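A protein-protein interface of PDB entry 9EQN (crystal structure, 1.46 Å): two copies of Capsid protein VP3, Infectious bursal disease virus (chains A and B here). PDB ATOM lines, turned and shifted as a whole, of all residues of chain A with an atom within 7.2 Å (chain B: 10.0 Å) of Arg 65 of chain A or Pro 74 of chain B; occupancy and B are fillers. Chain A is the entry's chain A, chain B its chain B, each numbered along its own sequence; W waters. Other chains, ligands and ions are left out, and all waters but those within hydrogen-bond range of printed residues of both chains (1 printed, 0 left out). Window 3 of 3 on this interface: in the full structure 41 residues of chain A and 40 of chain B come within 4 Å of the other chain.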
ATOM      1  N   PHE A  56      17.042  -3.386 -25.946  1.00  0.00           N
ATOM      2  CA  PHE A  56      18.420  -3.081 -25.568  1.00  0.00           C
ATOM      3  C   PHE A  56      19.144  -2.355 -26.692  1.00  0.00           C
ATOM      4  O   PHE A  56      19.866  -1.379 -26.449  1.00  0.00           O
ATOM      5  CB  PHE A  56      19.174  -4.360 -25.190  1.00  0.00           C
ATOM      6  CG  PHE A  56      20.645  -4.135 -24.898  1.00  0.00           C
ATOM      7  CD1 PHE A  56      21.580  -4.132 -25.925  1.00  0.00           C
ATOM      8  CD2 PHE A  56      21.084  -3.903 -23.613  1.00  0.00           C
ATOM      9  CE1 PHE A  56      22.921  -3.910 -25.682  1.00  0.00           C
ATOM     10  CE2 PHE A  56      22.429  -3.675 -23.361  1.00  0.00           C
ATOM     11  CZ  PHE A  56      23.349  -3.683 -24.402  1.00  0.00           C
ATOM     12  N   SER A  59      18.837   1.327 -26.785  1.00  0.00           N
ATOM     13  CA  SER A  59      19.657   2.016 -25.799  1.00  0.00           C
ATOM     14  C   SER A  59      21.143   1.920 -26.104  1.00  0.00           C
ATOM     15  O   SER A  59      21.942   2.611 -25.457  1.00  0.00           O
ATOM     16  CB  SER A  59      19.408   1.401 -24.418  1.00  0.00           C
ATOM     17  OG  SER A  59      20.080   0.151 -24.306  1.00  0.00           O
ATOM     18  N   ASP A  60      21.527   1.087 -27.075  1.00  0.00           N
ATOM     19  CA  ASP A  60      22.932   0.806 -27.371  1.00  0.00           C
ATOM     20  C   ASP A  60      23.118   0.813 -28.886  1.00  0.00           C
ATOM     21  O   ASP A  60      23.482  -0.198 -29.492  1.00  0.00           O
ATOM     22  CB  ASP A  60      23.322  -0.541 -26.757  1.00  0.00           C
ATOM     23  CG  ASP A  60      24.822  -0.768 -26.700  1.00  0.00           C
ATOM     24  OD1 ASP A  60      25.593   0.195 -26.440  1.00  0.00           O
ATOM     25  OD2 ASP A  60      25.222  -1.937 -26.872  1.00  0.00           O
ATOM     26  N   ASN A  62      25.242   1.864 -31.036  1.00  0.00           N
ATOM     27  CA  ASN A  62      26.546   1.546 -31.599  1.00  0.00           C
ATOM     28  C   ASN A  62      27.092   0.227 -31.076  1.00  0.00           C
ATOM     29  O   ASN A  62      28.252  -0.101 -31.343  1.00  0.00           O
ATOM     30  CB  ASN A  62      27.542   2.682 -31.348  1.00  0.00           C
ATOM     31  CG  ASN A  62      27.133   3.982 -32.032  1.00  0.00           C
ATOM     32  OD1 ASN A  62      26.240   4.687 -31.561  1.00  0.00           O
ATOM     33  ND2 ASN A  62      27.787   4.300 -33.146  1.00  0.00           N
ATOM     34  N   ALA A  63      26.276  -0.529 -30.336  1.00  0.00           N
ATOM     35  CA  ALA A  63      26.663  -1.808 -29.742  1.00  0.00           C
ATOM     36  C   ALA A  63      27.853  -1.672 -28.805  1.00  0.00           C
ATOM     37  O   ALA A  63      28.565  -2.642 -28.554  1.00  0.00           O
ATOM     38  CB  ALA A  63      26.913  -2.900 -30.794  1.00  0.00           C
ATOM     39  N   HIS A  64      28.072  -0.473 -28.271  1.00  0.00           N
ATOM     40  CA  HIS A  64      29.235  -0.245 -27.428  1.00  0.00           C
ATOM     41  C   HIS A  64      29.196  -1.112 -26.176  1.00  0.00           C
ATOM     42  O   HIS A  64      30.169  -1.802 -25.854  1.00  0.00           O
ATOM     43  CB  HIS A  64      29.281   1.232 -27.059  1.00  0.00           C
ATOM     44  CG  HIS A  64      30.427   1.593 -26.189  1.00  0.00           C
ATOM     45  ND1 HIS A  64      31.725   1.609 -26.642  1.00  0.00           N
ATOM     46  CD2 HIS A  64      30.473   1.959 -24.888  1.00  0.00           C
ATOM     47  CE1 HIS A  64      32.525   1.978 -25.658  1.00  0.00           C
ATOM     48  NE2 HIS A  64      31.790   2.200 -24.583  1.00  0.00           N
ATOM     49  N   ARG A  65      28.072  -1.090 -25.454  1.00  0.00           N
ATOM     50  CA  ARG A  65      27.962  -1.887 -24.238  1.00  0.00           C
ATOM     51  C   ARG A  65      27.912  -3.375 -24.550  1.00  0.00           C
ATOM     52  O   ARG A  65      28.520  -4.179 -23.836  1.00  0.00           O
ATOM     53  CB  ARG A  65      26.717  -1.478 -23.453  1.00  0.00           C
ATOM     54  CG  ARG A  65      26.521  -2.261 -22.166  1.00  0.00           C
ATOM     55  CD  ARG A  65      25.291  -1.786 -21.430  1.00  0.00           C
ATOM     56  NE  ARG A  65      25.266  -0.331 -21.323  1.00  0.00           N
ATOM     57  CZ  ARG A  65      25.812   0.353 -20.330  1.00  0.00           C
ATOM     58  NH1 ARG A  65      26.423  -0.257 -19.328  1.00  0.00           N
ATOM     59  NH2 ARG A  65      25.746   1.678 -20.344  1.00  0.00           N
ATOM     60  N   MET A  66      27.195  -3.760 -25.613  1.00  0.00           N
ATOM     61  CA  MET A  66      27.159  -5.169 -25.975  1.00  0.00           C
ATOM     62  C   MET A  66      28.535  -5.667 -26.394  1.00  0.00           C
ATOM     63  O   MET A  66      28.951  -6.762 -25.997  1.00  0.00           O
ATOM     64  CB  MET A  66      26.154  -5.410 -27.100  1.00  0.00           C
ATOM     65  CG  MET A  66      25.946  -6.893 -27.395  1.00  0.00           C
ATOM     66  SD  MET A  66      25.373  -7.849 -25.973  1.00  0.00           S
ATOM     67  CE  MET A  66      23.603  -7.604 -26.056  1.00  0.00           C
ATOM     68  N   ARG A  67      29.249  -4.884 -27.209  1.00  0.00           N
ATOM     69  CA  ARG A  67      30.553  -5.320 -27.692  1.00  0.00           C
ATOM     70  C   ARG A  67      31.512  -5.554 -26.535  1.00  0.00           C
ATOM     71  O   ARG A  67      32.290  -6.513 -26.552  1.00  0.00           O
ATOM     72  CB  ARG A  67      31.113  -4.275 -28.666  1.00  0.00           C
ATOM     73  CG  ARG A  67      32.372  -4.685 -29.378  1.00  0.00           C
ATOM     74  CD  ARG A  67      32.889  -3.551 -30.280  1.00  0.00           C
ATOM     75  NE  ARG A  67      31.992  -3.244 -31.387  1.00  0.00           N
ATOM     76  CZ  ARG A  67      31.190  -2.187 -31.470  1.00  0.00           C
ATOM     77  NH1 ARG A  67      31.183  -1.241 -30.538  1.00  0.00           N
ATOM     78  NH2 ARG A  67      30.378  -2.071 -32.521  1.00  0.00           N
ATOM     79  N   ASN A  68      31.441  -4.709 -25.502  1.00  0.00           N
ATOM     80  CA  ASN A  68      32.312  -4.897 -24.348  1.00  0.00           C
ATOM     81  C   ASN A  68      31.908  -6.116 -23.534  1.00  0.00           C
ATOM     82  O   ASN A  68      32.770  -6.806 -22.979  1.00  0.00           O
ATOM     83  CB  ASN A  68      32.316  -3.656 -23.460  1.00  0.00           C
ATOM     84  CG  ASN A  68      33.459  -3.658 -22.448  1.00  0.00           C
ATOM     85  OD1 ASN A  68      34.468  -4.349 -22.621  1.00  0.00           O
ATOM     86  ND2 ASN A  68      33.307  -2.873 -21.394  1.00  0.00           N
ATOM     87  N   PHE A  69      30.604  -6.388 -23.438  1.00  0.00           N
ATOM     88  CA  PHE A  69      30.149  -7.590 -22.754  1.00  0.00           C
ATOM     89  C   PHE A  69      30.632  -8.840 -23.475  1.00  0.00           C
ATOM     90  O   PHE A  69      31.169  -9.763 -22.854  1.00  0.00           O
ATOM     91  CB  PHE A  69      28.619  -7.583 -22.652  1.00  0.00           C
ATOM     92  CG  PHE A  69      28.031  -8.896 -22.213  1.00  0.00           C
ATOM     93  CD1 PHE A  69      28.209  -9.348 -20.921  1.00  0.00           C
ATOM     94  CD2 PHE A  69      27.290  -9.675 -23.088  1.00  0.00           C
ATOM     95  CE1 PHE A  69      27.673 -10.553 -20.512  1.00  0.00           C
ATOM     96  CE2 PHE A  69      26.754 -10.880 -22.680  1.00  0.00           C
ATOM     97  CZ  PHE A  69      26.946 -11.317 -21.385  1.00  0.00           C
ATOM     98  N   LEU A  70      30.448  -8.884 -24.797  1.00  0.00           N
ATOM     99  CA  LEU A  70      30.862 -10.057 -25.557  1.00  0.00           C
ATOM    100  C   LEU A  70      32.370 -10.250 -25.515  1.00  0.00           C
ATOM    101  O   LEU A  70      32.845 -11.393 -25.508  1.00  0.00           O
ATOM    102  CB  LEU A  70      30.373  -9.949 -27.001  1.00  0.00           C
ATOM    103  CG  LEU A  70      28.848  -9.918 -27.155  1.00  0.00           C
ATOM    104  CD1 LEU A  70      28.442  -9.699 -28.602  1.00  0.00           C
ATOM    105  CD2 LEU A  70      28.245 -11.207 -26.615  1.00  0.00           C
ATOM    106  N   ALA A  71      33.097  -9.145 -25.462  1.00  0.00           N
ATOM    107  CA  ALA A  71      34.564  -9.262 -25.529  1.00  0.00           C
ATOM    108  C   ALA A  71      35.063  -9.889 -24.244  1.00  0.00           C
ATOM    109  O   ALA A  71      35.990 -10.701 -24.319  1.00  0.00           O
ATOM    110  CB  ALA A  71      35.183  -7.915 -25.713  1.00  0.00           C
ATOM    111  N   TRP B  43      21.006  -4.551 -36.678  1.00  0.00           N
ATOM    112  CA  TRP B  43      21.873  -3.916 -35.692  1.00  0.00           C
ATOM    113  C   TRP B  43      23.149  -4.718 -35.484  1.00  0.00           C
ATOM    114  O   TRP B  43      24.232  -4.140 -35.333  1.00  0.00           O
ATOM    115  CB  TRP B  43      21.077  -3.757 -34.391  1.00  0.00           C
ATOM    116  CG  TRP B  43      21.800  -3.329 -33.134  1.00  0.00           C
ATOM    117  CD1 TRP B  43      22.142  -2.060 -32.770  1.00  0.00           C
ATOM    118  CD2 TRP B  43      22.148  -4.171 -32.030  1.00  0.00           C
ATOM    119  NE1 TRP B  43      22.732  -2.066 -31.519  1.00  0.00           N
ATOM    120  CE2 TRP B  43      22.744  -3.352 -31.045  1.00  0.00           C
ATOM    121  CE3 TRP B  43      22.039  -5.544 -31.791  1.00  0.00           C
ATOM    122  CZ2 TRP B  43      23.214  -3.858 -29.841  1.00  0.00           C
ATOM    123  CZ3 TRP B  43      22.506  -6.052 -30.591  1.00  0.00           C
ATOM    124  CH2 TRP B  43      23.097  -5.208 -29.632  1.00  0.00           C
ATOM    125  N   ASN B  47      26.905  -3.002 -36.794  1.00  0.00           N
ATOM    126  CA  ASN B  47      27.899  -2.761 -35.764  1.00  0.00           C
ATOM    127  C   ASN B  47      28.988  -3.812 -35.742  1.00  0.00           C
ATOM    128  O   ASN B  47      29.856  -3.776 -34.859  1.00  0.00           O
ATOM    129  CB  ASN B  47      27.217  -2.638 -34.398  1.00  0.00           C
ATOM    130  CG  ASN B  47      26.346  -1.403 -34.309  1.00  0.00           C
ATOM    131  OD1 ASN B  47      26.822  -0.280 -34.471  1.00  0.00           O
ATOM    132  ND2 ASN B  47      25.062  -1.602 -34.069  1.00  0.00           N
ATOM    133  N   ILE B  49      29.063  -7.118 -35.063  1.00  0.00           N
ATOM    134  CA  ILE B  49      29.128  -8.089 -33.969  1.00  0.00           C
ATOM    135  C   ILE B  49      28.388  -9.389 -34.281  1.00  0.00           C
ATOM    136  O   ILE B  49      27.959 -10.088 -33.361  1.00  0.00           O
ATOM    137  CB  ILE B  49      28.627  -7.491 -32.636  1.00  0.00           C
ATOM    138  CG1 ILE B  49      27.189  -6.957 -32.782  1.00  0.00           C
ATOM    139  CG2 ILE B  49      29.581  -6.423 -32.144  1.00  0.00           C
ATOM    140  CD1 ILE B  49      26.513  -6.714 -31.433  1.00  0.00           C
ATOM    141  N   MET B  53      28.361 -12.356 -31.570  1.00  0.00           N
ATOM    142  CA  MET B  53      27.125 -12.827 -30.966  1.00  0.00           C
ATOM    143  C   MET B  53      26.877 -14.295 -31.280  1.00  0.00           C
ATOM    144  O   MET B  53      26.381 -15.036 -30.425  1.00  0.00           O
ATOM    145  CB  MET B  53      25.949 -11.965 -31.423  1.00  0.00           C
ATOM    146  CG  MET B  53      24.680 -12.309 -30.705  1.00  0.00           C
ATOM    147  SD  MET B  53      24.723 -11.798 -28.989  1.00  0.00           S
ATOM    148  CE  MET B  53      24.474 -10.019 -29.161  1.00  0.00           C
ATOM    149  N   MET B  66      22.951 -14.312 -21.335  1.00  0.00           N
ATOM    150  CA  MET B  66      22.444 -13.139 -22.042  1.00  0.00           C
ATOM    151  C   MET B  66      21.246 -12.538 -21.318  1.00  0.00           C
ATOM    152  O   MET B  66      21.123 -11.309 -21.223  1.00  0.00           O
ATOM    153  CB  MET B  66      22.084 -13.486 -23.489  1.00  0.00           C
ATOM    154  CG  MET B  66      21.639 -12.269 -24.304  1.00  0.00           C
ATOM    155  SD  MET B  66      22.859 -10.931 -24.295  1.00  0.00           S
ATOM    156  CE  MET B  66      23.968 -11.512 -25.565  1.00  0.00           C
ATOM    157  N   ASN B  68      20.732 -12.530 -18.136  1.00  0.00           N
ATOM    158  CA  ASN B  68      21.242 -11.789 -16.987  1.00  0.00           C
ATOM    159  C   ASN B  68      21.850 -10.457 -17.401  1.00  0.00           C
ATOM    160  O   ASN B  68      21.679  -9.449 -16.703  1.00  0.00           O
ATOM    161  CB  ASN B  68      22.271 -12.619 -16.225  1.00  0.00           C
ATOM    162  CG  ASN B  68      22.813 -11.882 -15.012  1.00  0.00           C
ATOM    163  OD1 ASN B  68      23.920 -11.343 -15.036  1.00  0.00           O
ATOM    164  ND2 ASN B  68      22.017 -11.843 -13.950  1.00  0.00           N
ATOM    165  N   PHE B  69      22.578 -10.429 -18.522  1.00  0.00           N
ATOM    166  CA  PHE B  69      23.140  -9.167 -18.994  1.00  0.00           C
ATOM    167  C   PHE B  69      22.034  -8.171 -19.326  1.00  0.00           C
ATOM    168  O   PHE B  69      22.078  -7.007 -18.903  1.00  0.00           O
ATOM    169  CB  PHE B  69      24.030  -9.409 -20.217  1.00  0.00           C
ATOM    170  CG  PHE B  69      24.413  -8.146 -20.933  1.00  0.00           C
ATOM    171  CD1 PHE B  69      25.395  -7.317 -20.410  1.00  0.00           C
ATOM    172  CD2 PHE B  69      23.791  -7.777 -22.119  1.00  0.00           C
ATOM    173  CE1 PHE B  69      25.760  -6.143 -21.053  1.00  0.00           C
ATOM    174  CE2 PHE B  69      24.154  -6.600 -22.769  1.00  0.00           C
ATOM    175  CZ  PHE B  69      25.141  -5.786 -22.236  1.00  0.00           C
ATOM    176  N   LEU B  70      21.027  -8.621 -20.086  1.00  0.00           N
ATOM    177  CA  LEU B  70      19.910  -7.750 -20.443  1.00  0.00           C
ATOM    178  C   LEU B  70      19.155  -7.273 -19.204  1.00  0.00           C
ATOM    179  O   LEU B  70      18.726  -6.114 -19.133  1.00  0.00           O
ATOM    180  CB  LEU B  70      18.964  -8.471 -21.402  1.00  0.00           C
ATOM    181  CG  LEU B  70      19.506  -8.847 -22.786  1.00  0.00           C
ATOM    182  CD1 LEU B  70      18.517  -9.761 -23.512  1.00  0.00           C
ATOM    183  CD2 LEU B  70      19.784  -7.594 -23.599  1.00  0.00           C
ATOM    184  N   ALA B  71      18.999  -8.145 -18.209  1.00  0.00           N
ATOM    185  CA  ALA B  71      18.300  -7.765 -16.988  1.00  0.00           C
ATOM    186  C   ALA B  71      19.056  -6.688 -16.217  1.00  0.00           C
ATOM    187  O   ALA B  71      18.444  -5.867 -15.518  1.00  0.00           O
ATOM    188  CB  ALA B  71      18.098  -9.001 -16.117  1.00  0.00           C
ATOM    189  N   ASN B  72      20.377  -6.667 -16.328  1.00  0.00           N
ATOM    190  CA  ASN B  72      21.180  -5.723 -15.565  1.00  0.00           C
ATOM    191  C   ASN B  72      21.608  -4.504 -16.368  1.00  0.00           C
ATOM    192  O   ASN B  72      22.312  -3.643 -15.827  1.00  0.00           O
ATOM    193  CB  ASN B  72      22.403  -6.425 -14.970  1.00  0.00           C
ATOM    194  CG  ASN B  72      22.056  -7.296 -13.776  1.00  0.00           C
ATOM    195  OD1 ASN B  72      22.087  -6.838 -12.632  1.00  0.00           O
ATOM    196  ND2 ASN B  72      21.728  -8.560 -14.033  1.00  0.00           N
ATOM    197  N   ALA B  73      21.218  -4.410 -17.639  1.00  0.00           N
ATOM    198  CA  ALA B  73      21.535  -3.228 -18.419  1.00  0.00           C
ATOM    199  C   ALA B  73      20.895  -2.005 -17.764  1.00  0.00           C
ATOM    200  O   ALA B  73      19.824  -2.107 -17.158  1.00  0.00           O
ATOM    201  CB  ALA B  73      21.002  -3.382 -19.843  1.00  0.00           C
ATOM    202  N   PRO B  74      21.536  -0.839 -17.855  1.00  0.00           N
ATOM    203  CA  PRO B  74      21.000   0.351 -17.190  1.00  0.00           C
ATOM    204  C   PRO B  74      19.603   0.692 -17.684  1.00  0.00           C
ATOM    205  O   PRO B  74      19.187   0.322 -18.784  1.00  0.00           O
ATOM    206  CB  PRO B  74      22.005   1.450 -17.564  1.00  0.00           C
ATOM    207  CG  PRO B  74      23.272   0.712 -17.850  1.00  0.00           C
ATOM    208  CD  PRO B  74      22.846  -0.582 -18.481  1.00  0.00           C
ATOM    209  N   GLN B  75      18.829   1.233 -16.748  1.00  0.00           N
ATOM    210  CA  GLN B  75      17.438   1.609 -17.068  1.00  0.00           C
ATOM    211  C   GLN B  75      17.560   2.805 -18.005  1.00  0.00           C
ATOM    212  O   GLN B  75      18.642   3.413 -18.069  1.00  0.00           O
ATOM    213  CB  GLN B  75      16.639   1.880 -15.784  1.00  0.00           C
ATOM    214  CG  GLN B  75      17.265   2.887 -14.835  1.00  0.00           C
ATOM    215  CD  GLN B  75      16.414   3.069 -13.600  1.00  0.00           C
ATOM    216  OE1 GLN B  75      15.320   3.626 -13.651  1.00  0.00           O
ATOM    217  NE2 GLN B  75      16.914   2.587 -12.477  1.00  0.00           N
HETATM  218  O   HOH W   1      32.452  -4.968 -33.597  1.00  0.00           O
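Water W1 bridges the guanidinium group (NE) of Arg 67 of chain A (2.8 Å) and the backbone carbonyl oxygen (O) of Asn 47 of chain B (3.1 Å).
Met 66 of chain B touches its own counterpart, Met 66 of chain A. Met 66 of chain A touches Phe 69 of chain B, but with the chains exchanged Phe 69 of chain A does not touch Met 66 of chain B (4.1 Å). Phe 69 of chain A touches its own counterpart, Phe 69 of chain B. Positions printed for both chains: 66, 68, 69, 70 and 71. Of the 17 pairs that touch across the chains among the printed residues, 2 have their exchanged pair printed and touching as well.
The side-chain hydroxyl (OG) of Ser 59 of chain A is in hydrogen-bond range of the backbone carbonyl oxygen (O) of Phe 56 of chain A (2.6 Å). OD1 of Asp 60 of chain A sits at hydrogen-bond distance from N of His 64 of chain A. The side-chain carboxylate of Asp 60 of chain A sits at hydrogen-bond distance from the backbone NH of Arg 65 of chain A, at 3.0 Å. N of Met 66 of chain A is in hydrogen-bond range of OD2 of Asp 60 of chain A (3.0 Å). The backbone carbonyl oxygen (O) of Asn 62 of chain A lies within hydrogen-bond range of the guanidinium group (NH2) of Arg 67 of chain A. The backbone carbonyl oxygen (O) of Trp 43 of chain B lies within hydrogen-bond range of the side-chain amide nitrogen (ND2) of Asn 47 of chain B (3.0 Å).
His 64 of chain A touches none of the printed residues of chain B. Arg 65 of chain A touches just these residues of chain B: Phe 69 (3.8 Å) and Pro 74 (3.6 Å). Printed residues of chain A within 4 Å of Asn 47 of chain B: Asn 62, Ala 63 and Arg 67. Of the printed residues of chain A, Phe 69 of chain B touches Phe 56 (3.4 Å), Arg 65 (3.8 Å), Met 66 (3.5 Å) and Phe 69 (3.5 Å). Pro 74 of chain B touches just one residue of chain A: Arg 65 (3.6 Å). The nearest residue of chain A that does not touch Pro 74 of chain B is Ser 59 of chain A (5.6 Å).
Hydrophobic or aromatic side chains of chain A within 4 Å of the printed part of chain B: Phe 56, Ala 63, Met 66, Phe 69 and Leu 70. Among the printed residues, 17 pairs touch across the chains. Among the printed residues, no Asp or Glu carboxylate lies within 4 Å of a Lys or Arg side-chain nitrogen of the other chain.
O of Asp 60 of chain A is in hydrogen-bond range of NE1 of Trp 43 of chain B, 2.9 Å away. The backbone carbonyl oxygen (O) of Asn 62 of chain A sits close to the side-chain amide oxygen (OD1) of Asn 47 of chain B (3.4 Å). The backbone carbonyl oxygen (O) of Asn 47 of chain B sits at hydrogen-bond distance from the guanidinium group (NH2) of Arg 67 of chain A, 2.9 Å away.
Among the printed residues, merely in contact across the chains: Phe 56 of chain A with Phe 69 of chain B (3.4 Å), Met 66 of chain A with Phe 69 of chain B (3.5 Å), Phe 69 of chain A with Phe 69 of chain B (3.5 Å), Arg 65 of chain A with Pro 74 of chain B (3.6 Å), Ala 63 of chain A with Asn 47 of chain B (3.6 Å), Phe 56 of chain A with Leu 70 of chain B (3.7 Å), Arg 65 of chain A with Phe 69 of chain B (3.8 Å), Phe 56 of chain A with Ala 73 of chain B (3.8 Å), Met 66 of chain A with Met 66 of chain B (3.8 Å), Met 66 of chain A with Met 53 of chain B (3.9 Å), Ala 63 of chain A with Ile 49 of chain B (3.9 Å), Ala 63 of chain A with Trp 43 of chain B (3.9 Å), Met 66 of chain A with Trp 43 of chain B (3.97 Å) and Leu 70 of chain A with Met 53 of chain B (3.98 Å).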
